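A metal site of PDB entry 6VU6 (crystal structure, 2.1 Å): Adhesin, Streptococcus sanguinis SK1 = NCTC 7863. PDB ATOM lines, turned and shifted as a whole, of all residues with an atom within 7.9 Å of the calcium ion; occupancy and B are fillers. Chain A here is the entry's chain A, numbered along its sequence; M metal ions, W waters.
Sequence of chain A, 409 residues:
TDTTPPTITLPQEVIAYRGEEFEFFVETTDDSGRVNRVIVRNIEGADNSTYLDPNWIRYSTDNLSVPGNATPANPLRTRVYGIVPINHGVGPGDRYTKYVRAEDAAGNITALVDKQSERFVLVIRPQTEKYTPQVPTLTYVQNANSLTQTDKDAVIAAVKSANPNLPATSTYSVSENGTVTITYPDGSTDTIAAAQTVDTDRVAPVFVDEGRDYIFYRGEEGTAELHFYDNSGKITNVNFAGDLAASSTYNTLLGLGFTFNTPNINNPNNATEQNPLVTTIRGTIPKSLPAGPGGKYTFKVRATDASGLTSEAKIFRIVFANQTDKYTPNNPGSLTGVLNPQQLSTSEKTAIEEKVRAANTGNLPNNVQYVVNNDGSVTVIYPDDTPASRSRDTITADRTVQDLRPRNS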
ATOM      1  N   PRO A 126     -16.084  -3.149  15.804  1.00  0.00           N
ATOM      2  CA  PRO A 126     -16.094  -3.029  17.263  1.00  0.00           C
ATOM      3  C   PRO A 126     -15.610  -1.645  17.672  1.00  0.00           C
ATOM      4  O   PRO A 126     -14.910  -0.950  16.940  1.00  0.00           O
ATOM      5  CB  PRO A 126     -15.129  -4.125  17.736  1.00  0.00           C
ATOM      6  CG  PRO A 126     -14.272  -4.408  16.577  1.00  0.00           C
ATOM      7  CD  PRO A 126     -15.080  -4.115  15.334  1.00  0.00           C
ATOM      8  N   GLN A 127     -16.027  -1.247  18.869  1.00  0.00           N
ATOM      9  CA  GLN A 127     -15.718   0.084  19.374  1.00  0.00           C
ATOM     10  C   GLN A 127     -14.224   0.311  19.535  1.00  0.00           C
ATOM     11  O   GLN A 127     -13.748   1.453  19.452  1.00  0.00           O
ATOM     12  CB  GLN A 127     -16.429   0.305  20.698  1.00  0.00           C
ATOM     13  CG  GLN A 127     -17.850   0.746  20.593  1.00  0.00           C
ATOM     14  CD  GLN A 127     -18.434   1.050  21.952  1.00  0.00           C
ATOM     15  OE1 GLN A 127     -18.703   0.127  22.740  1.00  0.00           O
ATOM     16  NE2 GLN A 127     -18.619   2.326  22.256  1.00  0.00           N
ATOM     17  N   THR A 128     -13.459  -0.761  19.761  1.00  0.00           N
ATOM     18  CA  THR A 128     -12.018  -0.601  19.868  1.00  0.00           C
ATOM     19  C   THR A 128     -11.412  -0.100  18.556  1.00  0.00           C
ATOM     20  O   THR A 128     -10.425   0.638  18.580  1.00  0.00           O
ATOM     21  CB  THR A 128     -11.374  -1.928  20.327  1.00  0.00           C
ATOM     22  OG1 THR A 128      -9.964  -1.761  20.540  1.00  0.00           O
ATOM     23  CG2 THR A 128     -11.619  -3.062  19.362  1.00  0.00           C
ATOM     24  N   GLU A 129     -12.016  -0.444  17.412  1.00  0.00           N
ATOM     25  CA  GLU A 129     -11.505  -0.035  16.110  1.00  0.00           C
ATOM     26  C   GLU A 129     -11.736   1.448  15.842  1.00  0.00           C
ATOM     27  O   GLU A 129     -11.196   1.974  14.868  1.00  0.00           O
ATOM     28  CB  GLU A 129     -12.140  -0.849  14.994  1.00  0.00           C
ATOM     29  CG  GLU A 129     -11.632  -2.277  14.903  1.00  0.00           C
ATOM     30  CD  GLU A 129     -11.851  -2.879  13.531  1.00  0.00           C
ATOM     31  OE1 GLU A 129     -12.273  -2.131  12.624  1.00  0.00           O
ATOM     32  OE2 GLU A 129     -11.583  -4.089  13.355  1.00  0.00           O
ATOM     33  N   LYS A 130     -12.539   2.104  16.659  1.00  0.00           N
ATOM     34  CA  LYS A 130     -12.734   3.536  16.578  1.00  0.00           C
ATOM     35  C   LYS A 130     -11.750   4.315  17.443  1.00  0.00           C
ATOM     36  O   LYS A 130     -11.395   5.448  17.092  1.00  0.00           O
ATOM     37  CB  LYS A 130     -14.178   3.856  17.005  1.00  0.00           C
ATOM     38  CG  LYS A 130     -14.542   5.320  17.012  1.00  0.00           C
ATOM     39  CD  LYS A 130     -15.995   5.455  17.413  1.00  0.00           C
ATOM     40  CE  LYS A 130     -16.435   6.907  17.537  1.00  0.00           C
ATOM     41  NZ  LYS A 130     -17.660   7.010  18.386  1.00  0.00           N
ATOM     42  N   TYR A 131     -11.315   3.741  18.568  1.00  0.00           N
ATOM     43  CA  TYR A 131     -10.420   4.497  19.487  1.00  0.00           C
ATOM     44  C   TYR A 131      -8.986   3.956  19.546  1.00  0.00           C
ATOM     45  O   TYR A 131      -8.701   2.785  19.401  1.00  0.00           O
ATOM     46  CB  TYR A 131     -11.037   4.584  20.876  1.00  0.00           C
ATOM     47  CG  TYR A 131     -12.440   5.127  20.973  1.00  0.00           C
ATOM     48  CD1 TYR A 131     -12.708   6.475  20.959  1.00  0.00           C
ATOM     49  CD2 TYR A 131     -13.513   4.280  21.119  1.00  0.00           C
ATOM     50  CE1 TYR A 131     -14.006   6.956  21.072  1.00  0.00           C
ATOM     51  CE2 TYR A 131     -14.799   4.730  21.236  1.00  0.00           C
ATOM     52  CZ  TYR A 131     -15.044   6.074  21.221  1.00  0.00           C
ATOM     53  OH  TYR A 131     -16.317   6.509  21.307  1.00  0.00           O
ATOM     54  N   THR A 132      -8.064   4.900  19.728  1.00  0.00           N
ATOM     55  CA  THR A 132      -6.643   4.568  19.977  1.00  0.00           C
ATOM     56  C   THR A 132      -6.214   5.229  21.282  1.00  0.00           C
ATOM     57  O   THR A 132      -5.880   6.350  21.266  1.00  0.00           O
ATOM     58  CB  THR A 132      -5.663   4.958  18.873  1.00  0.00           C
ATOM     59  OG1 THR A 132      -6.290   4.753  17.610  1.00  0.00           O
ATOM     60  CG2 THR A 132      -4.446   4.082  18.893  1.00  0.00           C
ATOM     61  N   PRO A 133      -6.174   4.502  22.400  1.00  0.00           N
ATOM     62  CA  PRO A 133      -5.744   5.058  23.659  1.00  0.00           C
ATOM     63  C   PRO A 133      -4.378   5.747  23.640  1.00  0.00           C
ATOM     64  O   PRO A 133      -3.506   5.299  23.021  1.00  0.00           O
ATOM     65  CB  PRO A 133      -5.685   3.862  24.589  1.00  0.00           C
ATOM     66  CG  PRO A 133      -5.713   2.673  23.684  1.00  0.00           C
ATOM     67  CD  PRO A 133      -6.533   3.123  22.496  1.00  0.00           C
ATOM     68  N   LEU A 166     -12.352   8.679  25.389  1.00  0.00           N
ATOM     69  CA  LEU A 166     -12.865   7.328  25.462  1.00  0.00           C
ATOM     70  C   LEU A 166     -14.315   7.373  25.933  1.00  0.00           C
ATOM     71  O   LEU A 166     -14.722   8.341  26.581  1.00  0.00           O
ATOM     72  CB  LEU A 166     -12.005   6.472  26.397  1.00  0.00           C
ATOM     73  CG  LEU A 166     -10.608   6.116  25.865  1.00  0.00           C
ATOM     74  CD1 LEU A 166     -10.010   4.920  26.605  1.00  0.00           C
ATOM     75  CD2 LEU A 166     -10.653   5.878  24.356  1.00  0.00           C
ATOM     76  N   TYR A 184     -14.506  -1.493  26.454  1.00  0.00           N
ATOM     77  CA  TYR A 184     -15.503  -0.561  25.922  1.00  0.00           C
ATOM     78  C   TYR A 184     -16.905  -1.102  26.164  1.00  0.00           C
ATOM     79  O   TYR A 184     -17.067  -2.270  26.542  1.00  0.00           O
ATOM     80  CB  TYR A 184     -15.235  -0.337  24.438  1.00  0.00           C
ATOM     81  CG  TYR A 184     -13.893   0.287  24.185  1.00  0.00           C
ATOM     82  CD1 TYR A 184     -13.709   1.640  24.377  1.00  0.00           C
ATOM     83  CD2 TYR A 184     -12.789  -0.477  23.792  1.00  0.00           C
ATOM     84  CE1 TYR A 184     -12.487   2.227  24.172  1.00  0.00           C
ATOM     85  CE2 TYR A 184     -11.547   0.114  23.563  1.00  0.00           C
ATOM     86  CZ  TYR A 184     -11.406   1.481  23.763  1.00  0.00           C
ATOM     87  OH  TYR A 184     -10.221   2.145  23.563  1.00  0.00           O
ATOM     88  N   SER A 188     -15.484  -4.966  23.551  1.00  0.00           N
ATOM     89  CA  SER A 188     -14.196  -4.972  22.833  1.00  0.00           C
ATOM     90  C   SER A 188     -13.162  -4.288  23.715  1.00  0.00           C
ATOM     91  O   SER A 188     -13.510  -3.475  24.532  1.00  0.00           O
ATOM     92  CB  SER A 188     -14.287  -4.382  21.461  1.00  0.00           C
ATOM     93  OG  SER A 188     -14.511  -3.007  21.499  1.00  0.00           O
ATOM     94  N   THR A 189     -11.904  -4.605  23.473  1.00  0.00           N
ATOM     95  CA  THR A 189     -10.920  -4.112  24.456  1.00  0.00           C
ATOM     96  C   THR A 189      -9.743  -3.398  23.843  1.00  0.00           C
ATOM     97  O   THR A 189      -9.683  -3.195  22.637  1.00  0.00           O
ATOM     98  CB  THR A 189     -10.287  -5.299  25.190  1.00  0.00           C
ATOM     99  OG1 THR A 189      -9.939  -6.241  24.198  1.00  0.00           O
ATOM    100  CG2 THR A 189     -11.250  -5.945  26.164  1.00  0.00           C
ATOM    101  N   ASP A 190      -8.858  -3.049  24.741  1.00  0.00           N
ATOM    102  CA  ASP A 190      -7.624  -2.363  24.338  1.00  0.00           C
ATOM    103  C   ASP A 190      -6.614  -2.448  25.458  1.00  0.00           C
ATOM    104  O   ASP A 190      -6.983  -2.247  26.539  1.00  0.00           O
ATOM    105  CB  ASP A 190      -7.916  -0.919  24.064  1.00  0.00           C
ATOM    106  CG  ASP A 190      -7.332  -0.564  22.734  1.00  0.00           C
ATOM    107  OD1 ASP A 190      -6.638  -1.348  22.144  1.00  0.00           O
ATOM    108  OD2 ASP A 190      -7.660   0.477  22.289  1.00  0.00           O
ATOM    109  N   THR A 191      -5.362  -2.629  25.102  1.00  0.00           N
ATOM    110  CA  THR A 191      -4.329  -2.843  26.128  1.00  0.00           C
ATOM    111  C   THR A 191      -3.181  -1.847  26.034  1.00  0.00           C
ATOM    112  O   THR A 191      -2.717  -1.591  24.962  1.00  0.00           O
ATOM    113  CB  THR A 191      -3.691  -4.220  25.966  1.00  0.00           C
ATOM    114  OG1 THR A 191      -4.710  -5.193  26.156  1.00  0.00           O
ATOM    115  CG2 THR A 191      -2.608  -4.506  26.970  1.00  0.00           C
HETATM  116 CA    CA M   1      -8.435   0.408  19.742  1.00  0.00          CA
HETATM  117  O   HOH W   1      -7.749  -1.382  17.944  1.00  0.00           O
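N of Thr 128 lies within hydrogen-bond range of OG of Ser 188, 3.0 Å away. The side-chain hydroxyl (OG1) of Thr 128 lies close to the backbone carbonyl oxygen (O) of Thr 189. The side-chain amino group of Lys 130 is in hydrogen-bond range of the side-chain hydroxyl of Tyr 131 (3.3 Å). OH of Tyr 184 sits close to OD2 of Asp 190, 3.3 Å away.
Three residues have an atom within 4 Å of the calcium ion: Thr 128, Tyr 131 and Asp 190. The nearest printed residue that does not touch the calcium ion is Pro 133 (4.3 Å).
The calcium ion is bound by the backbone carbonyl oxygen (O) of Thr 128. The backbone carbonyl oxygen (O) of Tyr 131 binds the calcium ion (2.4 Å). Water W1 is bound to the calcium ion, at 2.6 Å. The calcium ion is bound by the side-chain carboxylate (OD2) of Asp 190 (2.7 Å). The side-chain hydroxyl (OG1) of Thr 128 binds the calcium ion, at 2.8 Å. The calcium ion has five donor atoms within binding distance.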
